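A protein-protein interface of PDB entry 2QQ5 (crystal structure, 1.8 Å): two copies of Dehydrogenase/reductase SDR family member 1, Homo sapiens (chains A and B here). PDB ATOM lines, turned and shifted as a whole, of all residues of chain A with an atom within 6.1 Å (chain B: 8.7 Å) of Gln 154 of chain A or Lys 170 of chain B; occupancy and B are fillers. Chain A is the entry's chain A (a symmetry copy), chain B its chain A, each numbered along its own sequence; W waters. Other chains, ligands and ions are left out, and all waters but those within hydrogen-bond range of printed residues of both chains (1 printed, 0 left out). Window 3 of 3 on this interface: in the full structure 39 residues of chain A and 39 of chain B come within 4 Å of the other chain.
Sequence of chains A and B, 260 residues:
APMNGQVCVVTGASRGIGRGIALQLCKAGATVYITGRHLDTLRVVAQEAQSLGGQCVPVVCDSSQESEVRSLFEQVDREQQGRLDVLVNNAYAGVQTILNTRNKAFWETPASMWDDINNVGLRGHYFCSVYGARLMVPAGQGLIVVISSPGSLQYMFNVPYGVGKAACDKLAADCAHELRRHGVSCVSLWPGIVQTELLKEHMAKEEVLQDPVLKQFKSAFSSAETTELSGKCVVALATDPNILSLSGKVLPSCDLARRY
Water W1 lies within hydrogen-bond range of the side-chain carboxylate (OD2) of Asp 174 of chain B (2.7 Å), the backbone NH (N) of Met 156 of chain A (2.9 Å) and the backbone NH (N) of Gly 162 of chain A (3.5 Å).
Positions printed for both chains: 152, 163, 164, 165 and 166.
Of the 14 printed residues of chain A, 8 touch a printed residue of chain B. Hydrophobic or aromatic side chains of chain A within 4 Å of the printed part of chain B: Tyr 155, Val 159, Val 163 and Ala 166. Among the printed residues, no Asp or Glu carboxylate lies within 4 Å of a Lys or Arg side-chain nitrogen of the other chain.
Among the printed residues, pairs that only touch across the chains: Val 163 of chain A with Ala 167 of chain B (3.4 Å), Tyr 155 of chain A with His 177 of chain B (3.4 Å), Val 163 of chain A with Leu 171 of chain B (3.5 Å), Tyr 155 of chain A with Asp 174 of chain B (3.5 Å), Ala 166 of chain A with Lys 170 of chain B (3.6 Å), Gly 162 of chain A with Asp 174 of chain B (3.7 Å), Val 163 of chain A with Lys 170 of chain B (3.7 Å), Val 163 of chain A with Asp 174 of chain B (3.8 Å), Val 159 of chain A with Leu 171 of chain B (3.9 Å), Val 159 of chain A with Asp 174 of chain B (3.9 Å) and Ser 152 of chain A with Lys 170 of chain B (3.9 Å).
The side-chain amino group (NZ) of Lys 170 of chain B lies within hydrogen-bond range of the backbone carbonyl oxygen (O) of Gln 154 of chain A. The side-chain amino group of Lys 170 of chain B is in hydrogen-bond range of the backbone carbonyl oxygen of Gly 162 of chain A. The backbone carbonyl oxygen of Gly 151 of chain A is in hydrogen-bond range of the side-chain amino group of Lys 170 of chain B, at 2.8 Å.
Of the printed residues of chain B, Gln 154 of chain A touches Lys 170. Of the printed residues of chain B, Val 159 of chain A touches Leu 171 (3.9 Å) and Asp 174 (3.9 Å). Printed residues of chain B within 4 Å of Ala 166 of chain A: Lys 170. Printed residues of chain B within 4 Å of Tyr 155 of chain A: Asp 174 and His 177. Ser 188 of chain B touches none of the printed residues of chain A. The nearest residue of chain B that does not touch Gln 154 of chain A is Asp 174 of chain B (4.1 Å). The nearest printed residue of chain B that does not touch Ala 166 of chain A is Ala 166 of chain B (4.3 Å).
The side-chain amino group of Lys 170 of chain B is in salt-bridge range of the side-chain carboxylate of Asp 174 of chain B (2.6 Å). The backbone carbonyl oxygen of Leu 171 of chain B lies close to the side-chain sulfur of Cys 175 of chain B (3.3 Å).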
ATOM      1  N   PRO A 150      33.580 -19.913   8.662  1.00  0.00           N
ATOM      2  CA  PRO A 150      32.697 -20.999   8.212  1.00  0.00           C
ATOM      3  C   PRO A 150      31.423 -20.539   7.501  1.00  0.00           C
ATOM      4  O   PRO A 150      30.733 -21.349   6.894  1.00  0.00           O
ATOM      5  CB  PRO A 150      32.320 -21.743   9.503  1.00  0.00           C
ATOM      6  CG  PRO A 150      33.206 -21.258  10.537  1.00  0.00           C
ATOM      7  CD  PRO A 150      33.818 -19.954  10.113  1.00  0.00           C
ATOM      8  N   GLY A 151      31.117 -19.251   7.548  1.00  0.00           N
ATOM      9  CA  GLY A 151      30.063 -18.713   6.716  1.00  0.00           C
ATOM     10  C   GLY A 151      30.277 -18.977   5.239  1.00  0.00           C
ATOM     11  O   GLY A 151      29.325 -18.929   4.475  1.00  0.00           O
ATOM     12  N   SER A 152      31.515 -19.290   4.829  1.00  0.00           N
ATOM     13  CA  SER A 152      31.760 -19.747   3.457  1.00  0.00           C
ATOM     14  C   SER A 152      31.077 -21.095   3.117  1.00  0.00           C
ATOM     15  O   SER A 152      30.849 -21.368   1.939  1.00  0.00           O
ATOM     16  CB  SER A 152      33.271 -19.890   3.216  1.00  0.00           C
ATOM     17  OG  SER A 152      33.764 -20.963   4.015  1.00  0.00           O
ATOM     18  N   LEU A 153      30.765 -21.914   4.136  1.00  0.00           N
ATOM     19  CA  LEU A 153      30.270 -23.274   3.944  1.00  0.00           C
ATOM     20  C   LEU A 153      28.773 -23.415   4.028  1.00  0.00           C
ATOM     21  O   LEU A 153      28.216 -24.433   3.615  1.00  0.00           O
ATOM     22  CB  LEU A 153      30.845 -24.208   5.024  1.00  0.00           C
ATOM     23  CG  LEU A 153      32.360 -24.258   5.139  1.00  0.00           C
ATOM     24  CD1 LEU A 153      32.753 -25.238   6.256  1.00  0.00           C
ATOM     25  CD2 LEU A 153      32.955 -24.638   3.796  1.00  0.00           C
ATOM     26  N   GLN A 154      28.125 -22.447   4.655  1.00  0.00           N
ATOM     27  CA  GLN A 154      26.759 -22.659   5.149  1.00  0.00           C
ATOM     28  C   GLN A 154      26.162 -21.325   5.507  1.00  0.00           C
ATOM     29  O   GLN A 154      26.877 -20.322   5.572  1.00  0.00           O
ATOM     30  CB  GLN A 154      26.781 -23.564   6.389  1.00  0.00           C
ATOM     31  CG  GLN A 154      27.591 -22.969   7.548  1.00  0.00           C
ATOM     32  CD  GLN A 154      28.319 -24.017   8.401  1.00  0.00           C
ATOM     33  OE1 GLN A 154      28.425 -25.193   8.031  1.00  0.00           O
ATOM     34  NE2 GLN A 154      28.812 -23.587   9.549  1.00  0.00           N
ATOM     35  N   TYR A 155      24.862 -21.330   5.773  1.00  0.00           N
ATOM     36  CA  TYR A 155      24.192 -20.111   6.187  1.00  0.00           C
ATOM     37  C   TYR A 155      24.751 -19.680   7.530  1.00  0.00           C
ATOM     38  O   TYR A 155      24.862 -20.486   8.462  1.00  0.00           O
ATOM     39  CB  TYR A 155      22.696 -20.337   6.309  1.00  0.00           C
ATOM     40  CG  TYR A 155      21.934 -19.102   6.704  1.00  0.00           C
ATOM     41  CD1 TYR A 155      21.460 -18.220   5.734  1.00  0.00           C
ATOM     42  CD2 TYR A 155      21.684 -18.810   8.053  1.00  0.00           C
ATOM     43  CE1 TYR A 155      20.756 -17.069   6.095  1.00  0.00           C
ATOM     44  CE2 TYR A 155      20.995 -17.654   8.419  1.00  0.00           C
ATOM     45  CZ  TYR A 155      20.525 -16.802   7.437  1.00  0.00           C
ATOM     46  OH  TYR A 155      19.828 -15.661   7.810  1.00  0.00           O
ATOM     47  N   MET A 156      25.125 -18.411   7.612  1.00  0.00           N
ATOM     48  CA  MET A 156      25.566 -17.806   8.869  1.00  0.00           C
ATOM     49  C   MET A 156      25.163 -16.333   8.954  1.00  0.00           C
ATOM     50  O   MET A 156      25.518 -15.537   8.092  1.00  0.00           O
ATOM     51  CB  MET A 156      27.078 -17.910   9.004  1.00  0.00           C
ATOM     52  CG  MET A 156      27.588 -17.441  10.378  1.00  0.00           C
ATOM     53  N   VAL A 159      22.259 -13.211   4.701  1.00  0.00           N
ATOM     54  CA  VAL A 159      22.601 -13.585   3.346  1.00  0.00           C
ATOM     55  C   VAL A 159      23.886 -12.921   2.862  1.00  0.00           C
ATOM     56  O   VAL A 159      24.813 -13.608   2.415  1.00  0.00           O
ATOM     57  CB  VAL A 159      21.430 -13.399   2.377  1.00  0.00           C
ATOM     58  CG1 VAL A 159      21.864 -13.676   0.931  1.00  0.00           C
ATOM     59  CG2 VAL A 159      20.264 -14.328   2.800  1.00  0.00           C
ATOM     60  N   TYR A 161      26.357 -11.601   4.414  1.00  0.00           N
ATOM     61  CA  TYR A 161      27.528 -12.080   5.153  1.00  0.00           C
ATOM     62  C   TYR A 161      28.067 -13.399   4.574  1.00  0.00           C
ATOM     63  O   TYR A 161      29.268 -13.518   4.231  1.00  0.00           O
ATOM     64  CB  TYR A 161      27.211 -12.255   6.644  1.00  0.00           C
ATOM     65  CG  TYR A 161      28.364 -12.829   7.441  1.00  0.00           C
ATOM     66  CD1 TYR A 161      29.379 -12.015   7.929  1.00  0.00           C
ATOM     67  CD2 TYR A 161      28.450 -14.205   7.677  1.00  0.00           C
ATOM     68  CE1 TYR A 161      30.458 -12.557   8.628  1.00  0.00           C
ATOM     69  CE2 TYR A 161      29.499 -14.752   8.380  1.00  0.00           C
ATOM     70  CZ  TYR A 161      30.506 -13.930   8.860  1.00  0.00           C
ATOM     71  OH  TYR A 161      31.557 -14.530   9.542  1.00  0.00           O
ATOM     72  N   GLY A 162      27.193 -14.395   4.510  1.00  0.00           N
ATOM     73  CA  GLY A 162      27.531 -15.747   4.011  1.00  0.00           C
ATOM     74  C   GLY A 162      27.974 -15.802   2.573  1.00  0.00           C
ATOM     75  O   GLY A 162      28.903 -16.530   2.219  1.00  0.00           O
ATOM     76  N   VAL A 163      27.310 -15.035   1.727  1.00  0.00           N
ATOM     77  CA  VAL A 163      27.686 -14.945   0.333  1.00  0.00           C
ATOM     78  C   VAL A 163      29.089 -14.344   0.221  1.00  0.00           C
ATOM     79  O   VAL A 163      29.934 -14.851  -0.531  1.00  0.00           O
ATOM     80  CB  VAL A 163      26.668 -14.143  -0.480  1.00  0.00           C
ATOM     81  CG1 VAL A 163      27.190 -13.899  -1.927  1.00  0.00           C
ATOM     82  CG2 VAL A 163      25.254 -14.863  -0.503  1.00  0.00           C
ATOM     83  N   GLY A 164      29.338 -13.278   0.985  1.00  0.00           N
ATOM     84  CA  GLY A 164      30.627 -12.630   1.008  1.00  0.00           C
ATOM     85  C   GLY A 164      31.741 -13.556   1.452  1.00  0.00           C
ATOM     86  O   GLY A 164      32.850 -13.525   0.898  1.00  0.00           O
ATOM     87  N   LYS A 165      31.453 -14.355   2.471  1.00  0.00           N
ATOM     88  CA  LYS A 165      32.434 -15.326   2.992  1.00  0.00           C
ATOM     89  C   LYS A 165      32.718 -16.444   1.992  1.00  0.00           C
ATOM     90  O   LYS A 165      33.873 -16.819   1.819  1.00  0.00           O
ATOM     91  CB  LYS A 165      32.014 -15.889   4.359  1.00  0.00           C
ATOM     92  CG  LYS A 165      32.026 -14.847   5.484  1.00  0.00           C
ATOM     93  CD  LYS A 165      33.452 -14.448   5.849  1.00  0.00           C
ATOM     94  CE  LYS A 165      33.526 -13.393   6.940  1.00  0.00           C
ATOM     95  NZ  LYS A 165      33.500 -12.027   6.381  1.00  0.00           N
ATOM     96  N   ALA A 166      31.684 -16.966   1.331  1.00  0.00           N
ATOM     97  CA  ALA A 166      31.889 -17.916   0.217  1.00  0.00           C
ATOM     98  C   ALA A 166      32.812 -17.281  -0.828  1.00  0.00           C
ATOM     99  O   ALA A 166      33.770 -17.924  -1.280  1.00  0.00           O
ATOM    100  CB  ALA A 166      30.558 -18.333  -0.410  1.00  0.00           C
ATOM    101  N   LEU B 122      26.615  -9.945  -9.912  1.00  0.00           N
ATOM    102  CA  LEU B 122      26.518 -10.451  -8.528  1.00  0.00           C
ATOM    103  C   LEU B 122      25.700  -9.514  -7.679  1.00  0.00           C
ATOM    104  O   LEU B 122      24.609  -9.883  -7.196  1.00  0.00           O
ATOM    105  CB  LEU B 122      27.908 -10.716  -7.925  1.00  0.00           C
ATOM    106  CG  LEU B 122      27.905 -11.224  -6.474  1.00  0.00           C
ATOM    107  CD1 LEU B 122      27.160 -12.555  -6.374  1.00  0.00           C
ATOM    108  CD2 LEU B 122      29.370 -11.345  -5.951  1.00  0.00           C
ATOM    109  N   VAL B 146      18.891 -18.448  -9.831  1.00  0.00           N
ATOM    110  CA  VAL B 146      20.197 -17.849 -10.052  1.00  0.00           C
ATOM    111  C   VAL B 146      20.959 -18.659 -11.086  1.00  0.00           C
ATOM    112  O   VAL B 146      21.118 -19.882 -10.941  1.00  0.00           O
ATOM    113  CB  VAL B 146      21.011 -17.767  -8.739  1.00  0.00           C
ATOM    114  CG1 VAL B 146      22.353 -17.086  -8.987  1.00  0.00           C
ATOM    115  CG2 VAL B 146      20.209 -17.033  -7.657  1.00  0.00           C
ATOM    116  N   SER B 148      24.191 -19.943 -12.649  1.00  0.00           N
ATOM    117  CA  SER B 148      25.587 -20.119 -12.204  1.00  0.00           C
ATOM    118  C   SER B 148      26.281 -21.186 -13.055  1.00  0.00           C
ATOM    119  O   SER B 148      25.810 -21.498 -14.172  1.00  0.00           O
ATOM    120  CB  SER B 148      25.628 -20.464 -10.702  1.00  0.00           C
ATOM    121  OG  SER B 148      26.965 -20.426 -10.184  1.00  0.00           O
ATOM    122  N   SER B 152      31.671 -22.150  -9.626  1.00  0.00           N
ATOM    123  CA  SER B 152      31.460 -22.085  -8.176  1.00  0.00           C
ATOM    124  C   SER B 152      32.341 -23.073  -7.372  1.00  0.00           C
ATOM    125  O   SER B 152      32.572 -22.837  -6.187  1.00  0.00           O
ATOM    126  CB  SER B 152      29.985 -22.369  -7.850  1.00  0.00           C
ATOM    127  OG  SER B 152      29.698 -23.730  -8.165  1.00  0.00           O
ATOM    128  N   VAL B 163      35.026 -16.414  -8.511  1.00  0.00           N
ATOM    129  CA  VAL B 163      34.596 -15.864  -7.243  1.00  0.00           C
ATOM    130  C   VAL B 163      33.111 -15.502  -7.323  1.00  0.00           C
ATOM    131  O   VAL B 163      32.335 -15.815  -6.408  1.00  0.00           O
ATOM    132  CB  VAL B 163      35.443 -14.659  -6.829  1.00  0.00           C
ATOM    133  CG1 VAL B 163      34.842 -13.972  -5.567  1.00  0.00           C
ATOM    134  CG2 VAL B 163      36.954 -15.076  -6.581  1.00  0.00           C
ATOM    135  N   GLY B 164      32.717 -14.861  -8.427  1.00  0.00           N
ATOM    136  CA  GLY B 164      31.341 -14.490  -8.652  1.00  0.00           C
ATOM    137  C   GLY B 164      30.407 -15.682  -8.675  1.00  0.00           C
ATOM    138  O   GLY B 164      29.291 -15.624  -8.139  1.00  0.00           O
ATOM    139  N   LYS B 165      30.854 -16.751  -9.323  1.00  0.00           N
ATOM    140  CA  LYS B 165      30.062 -17.992  -9.404  1.00  0.00           C
ATOM    141  C   LYS B 165      29.930 -18.676  -8.045  1.00  0.00           C
ATOM    142  O   LYS B 165      28.847 -19.140  -7.706  1.00  0.00           O
ATOM    143  CB  LYS B 165      30.610 -18.955 -10.468  1.00  0.00           C
ATOM    144  CG  LYS B 165      30.466 -18.437 -11.903  1.00  0.00           C
ATOM    145  CD  LYS B 165      29.007 -18.443 -12.346  1.00  0.00           C
ATOM    146  CE  LYS B 165      28.797 -17.909 -13.752  1.00  0.00           C
ATOM    147  NZ  LYS B 165      28.583 -16.448 -13.756  1.00  0.00           N
ATOM    148  N   ALA B 166      31.013 -18.733  -7.270  1.00  0.00           N
ATOM    149  CA  ALA B 166      30.930 -19.208  -5.872  1.00  0.00           C
ATOM    150  C   ALA B 166      29.882 -18.382  -5.117  1.00  0.00           C
ATOM    151  O   ALA B 166      29.028 -18.953  -4.424  1.00  0.00           O
ATOM    152  CB  ALA B 166      32.290 -19.133  -5.177  1.00  0.00           C
ATOM    153  N   ALA B 167      29.925 -17.055  -5.279  1.00  0.00           N
ATOM    154  CA  ALA B 167      28.990 -16.185  -4.599  1.00  0.00           C
ATOM    155  C   ALA B 167      27.544 -16.424  -5.040  1.00  0.00           C
ATOM    156  O   ALA B 167      26.624 -16.385  -4.218  1.00  0.00           O
ATOM    157  CB  ALA B 167      29.369 -14.702  -4.798  1.00  0.00           C
ATOM    158  N   CYS B 168      27.336 -16.618  -6.335  1.00  0.00           N
ATOM    159  CA  CYS B 168      25.983 -16.881  -6.875  1.00  0.00           C
ATOM    160  C   CYS B 168      25.378 -18.185  -6.335  1.00  0.00           C
ATOM    161  O   CYS B 168      24.181 -18.241  -5.986  1.00  0.00           O
ATOM    162  CB  CYS B 168      25.989 -16.903  -8.430  1.00  0.00           C
ATOM    163  SG  CYS B 168      26.236 -15.319  -9.214  1.00  0.00           S
ATOM    164  N   ASP B 169      26.175 -19.253  -6.277  1.00  0.00           N
ATOM    165  CA  ASP B 169      25.664 -20.519  -5.741  1.00  0.00           C
ATOM    166  C   ASP B 169      25.296 -20.321  -4.267  1.00  0.00           C
ATOM    167  O   ASP B 169      24.272 -20.836  -3.792  1.00  0.00           O
ATOM    168  CB  ASP B 169      26.692 -21.656  -5.885  1.00  0.00           C
ATOM    169  CG  ASP B 169      26.578 -22.443  -7.202  1.00  0.00           C
ATOM    170  OD1 ASP B 169      25.807 -22.083  -8.121  1.00  0.00           O
ATOM    171  OD2 ASP B 169      27.281 -23.467  -7.294  1.00  0.00           O
ATOM    172  N   LYS B 170      26.122 -19.565  -3.537  1.00  0.00           N
ATOM    173  CA  LYS B 170      25.838 -19.317  -2.123  1.00  0.00           C
ATOM    174  C   LYS B 170      24.599 -18.449  -1.925  1.00  0.00           C
ATOM    175  O   LYS B 170      23.821 -18.667  -0.980  1.00  0.00           O
ATOM    176  CB  LYS B 170      27.054 -18.721  -1.430  1.00  0.00           C
ATOM    177  CG  LYS B 170      26.957 -18.575   0.070  1.00  0.00           C
ATOM    178  CD  LYS B 170      26.564 -19.886   0.767  1.00  0.00           C
ATOM    179  CE  LYS B 170      27.235 -20.001   2.136  1.00  0.00           C
ATOM    180  NZ  LYS B 170      26.913 -18.917   3.044  1.00  0.00           N
ATOM    181  N   LEU B 171      24.435 -17.460  -2.804  1.00  0.00           N
ATOM    182  CA  LEU B 171      23.274 -16.590  -2.800  1.00  0.00           C
ATOM    183  C   LEU B 171      22.010 -17.414  -2.929  1.00  0.00           C
ATOM    184  O   LEU B 171      21.062 -17.228  -2.178  1.00  0.00           O
ATOM    185  CB  LEU B 171      23.334 -15.574  -3.947  1.00  0.00           C
ATOM    186  CG  LEU B 171      22.155 -14.590  -4.115  1.00  0.00           C
ATOM    187  CD1 LEU B 171      22.064 -13.628  -2.914  1.00  0.00           C
ATOM    188  CD2 LEU B 171      22.337 -13.842  -5.440  1.00  0.00           C
ATOM    189  N   ALA B 172      21.989 -18.322  -3.895  1.00  0.00           N
ATOM    190  CA  ALA B 172      20.843 -19.225  -4.023  1.00  0.00           C
ATOM    191  C   ALA B 172      20.573 -20.037  -2.753  1.00  0.00           C
ATOM    192  O   ALA B 172      19.436 -20.088  -2.278  1.00  0.00           O
ATOM    193  CB  ALA B 172      20.998 -20.145  -5.249  1.00  0.00           C
ATOM    194  N   ALA B 173      21.615 -20.654  -2.192  1.00  0.00           N
ATOM    195  CA  ALA B 173      21.482 -21.485  -1.002  1.00  0.00           C
ATOM    196  C   ALA B 173      20.985 -20.695   0.224  1.00  0.00           C
ATOM    197  O   ALA B 173      20.071 -21.123   0.964  1.00  0.00           O
ATOM    198  CB  ALA B 173      22.822 -22.147  -0.691  1.00  0.00           C
ATOM    199  N   ASP B 174      21.594 -19.545   0.450  1.00  0.00           N
ATOM    200  CA  ASP B 174      21.283 -18.766   1.653  1.00  0.00           C
ATOM    201  C   ASP B 174      19.893 -18.089   1.544  1.00  0.00           C
ATOM    202  O   ASP B 174      19.148 -18.014   2.518  1.00  0.00           O
ATOM    203  CB  ASP B 174      22.382 -17.752   1.896  1.00  0.00           C
ATOM    204  CG  ASP B 174      23.675 -18.386   2.468  1.00  0.00           C
ATOM    205  OD1 ASP B 174      23.719 -19.615   2.717  1.00  0.00           O
ATOM    206  OD2 ASP B 174      24.658 -17.641   2.662  1.00  0.00           O
ATOM    207  N   CYS B 175      19.537 -17.590   0.354  1.00  0.00           N
ATOM    208  CA  CYS B 175      18.178 -17.082   0.124  1.00  0.00           C
ATOM    209  C   CYS B 175      17.140 -18.189   0.311  1.00  0.00           C
ATOM    210  O   CYS B 175      16.100 -17.968   0.949  1.00  0.00           O
ATOM    211  CB  CYS B 175      18.041 -16.476  -1.283  1.00  0.00           C
ATOM    212  SG  CYS B 175      18.896 -14.904  -1.456  1.00  0.00           S
ATOM    213  N   ALA B 176      17.419 -19.368  -0.260  1.00  0.00           N
ATOM    214  CA  ALA B 176      16.565 -20.551  -0.078  1.00  0.00           C
ATOM    215  C   ALA B 176      16.302 -20.803   1.405  1.00  0.00           C
ATOM    216  O   ALA B 176      15.162 -21.069   1.833  1.00  0.00           O
ATOM    217  CB  ALA B 176      17.212 -21.803  -0.742  1.00  0.00           C
ATOM    218  N   HIS B 177      17.377 -20.750   2.182  1.00  0.00           N
ATOM    219  CA  HIS B 177      17.296 -21.025   3.609  1.00  0.00           C
ATOM    220  C   HIS B 177      16.261 -20.138   4.304  1.00  0.00           C
ATOM    221  O   HIS B 177      15.405 -20.620   5.078  1.00  0.00           O
ATOM    222  CB  HIS B 177      18.682 -20.832   4.231  1.00  0.00           C
ATOM    223  CG  HIS B 177      18.712 -21.105   5.695  1.00  0.00           C
ATOM    224  ND1 HIS B 177      18.643 -20.104   6.639  1.00  0.00           N
ATOM    225  CD2 HIS B 177      18.781 -22.267   6.378  1.00  0.00           C
ATOM    226  CE1 HIS B 177      18.665 -20.642   7.846  1.00  0.00           C
ATOM    227  NE2 HIS B 177      18.770 -21.951   7.716  1.00  0.00           N
ATOM    228  N   CYS B 186      14.251 -21.105  -4.106  1.00  0.00           N
ATOM    229  CA  CYS B 186      15.374 -20.445  -4.785  1.00  0.00           C
ATOM    230  C   CYS B 186      16.392 -21.508  -5.173  1.00  0.00           C
ATOM    231  O   CYS B 186      16.813 -22.308  -4.332  1.00  0.00           O
ATOM    232  CB  CYS B 186      15.984 -19.367  -3.883  1.00  0.00           C
ATOM    233  SG  CYS B 186      17.346 -18.459  -4.636  1.00  0.00           S
ATOM    234  N   SER B 188      19.884 -22.752  -7.883  1.00  0.00           N
ATOM    235  CA  SER B 188      20.959 -22.350  -8.756  1.00  0.00           C
ATOM    236  C   SER B 188      20.915 -23.256  -9.981  1.00  0.00           C
ATOM    237  O   SER B 188      21.008 -24.483  -9.872  1.00  0.00           O
ATOM    238  CB  SER B 188      22.312 -22.471  -8.058  1.00  0.00           C
ATOM    239  OG  SER B 188      23.317 -22.190  -8.995  1.00  0.00           O
ATOM    240  N   TRP B 190      22.581 -24.427 -13.484  1.00  0.00           N
ATOM    241  CA  TRP B 190      23.805 -24.440 -14.322  1.00  0.00           C
ATOM    242  C   TRP B 190      23.387 -24.846 -15.741  1.00  0.00           C
ATOM    243  O   TRP B 190      23.223 -26.054 -16.049  1.00  0.00           O
ATOM    244  CB  TRP B 190      24.802 -25.471 -13.808  1.00  0.00           C
ATOM    245  CG  TRP B 190      25.430 -25.172 -12.489  1.00  0.00           C
ATOM    246  CD1 TRP B 190      25.177 -24.126 -11.637  1.00  0.00           C
ATOM    247  CD2 TRP B 190      26.431 -25.975 -11.854  1.00  0.00           C
ATOM    248  NE1 TRP B 190      25.972 -24.232 -10.516  1.00  0.00           N
ATOM    249  CE2 TRP B 190      26.751 -25.358 -10.626  1.00  0.00           C
ATOM    250  CE3 TRP B 190      27.093 -27.147 -12.217  1.00  0.00           C
ATOM    251  CZ2 TRP B 190      27.691 -25.896  -9.744  1.00  0.00           C
ATOM    252  CZ3 TRP B 190      28.036 -27.676 -11.346  1.00  0.00           C
ATOM    253  CH2 TRP B 190      28.321 -27.049 -10.122  1.00  0.00           C
ATOM    254  N   GLY B 248      17.298 -24.525  -2.866  1.00  0.00           N
ATOM    255  CA  GLY B 248      18.609 -24.426  -2.243  1.00  0.00           C
ATOM    256  C   GLY B 248      19.632 -25.295  -2.970  1.00  0.00           C
ATOM    257  O   GLY B 248      20.810 -25.267  -2.644  1.00  0.00           O
ATOM    258  N   VAL B 250      21.800 -26.860  -6.403  1.00  0.00           N
ATOM    259  CA  VAL B 250      22.380 -26.710  -7.729  1.00  0.00           C
ATOM    260  C   VAL B 250      21.736 -27.735  -8.678  1.00  0.00           C
ATOM    261  O   VAL B 250      21.639 -28.951  -8.368  1.00  0.00           O
ATOM    262  CB  VAL B 250      23.915 -26.959  -7.703  1.00  0.00           C
ATOM    263  CG1 VAL B 250      24.474 -27.073  -9.142  1.00  0.00           C
ATOM    264  CG2 VAL B 250      24.651 -25.867  -6.938  1.00  0.00           C
HETATM  265  O   HOH W   1      24.778 -16.797   5.251  1.00  0.00           O
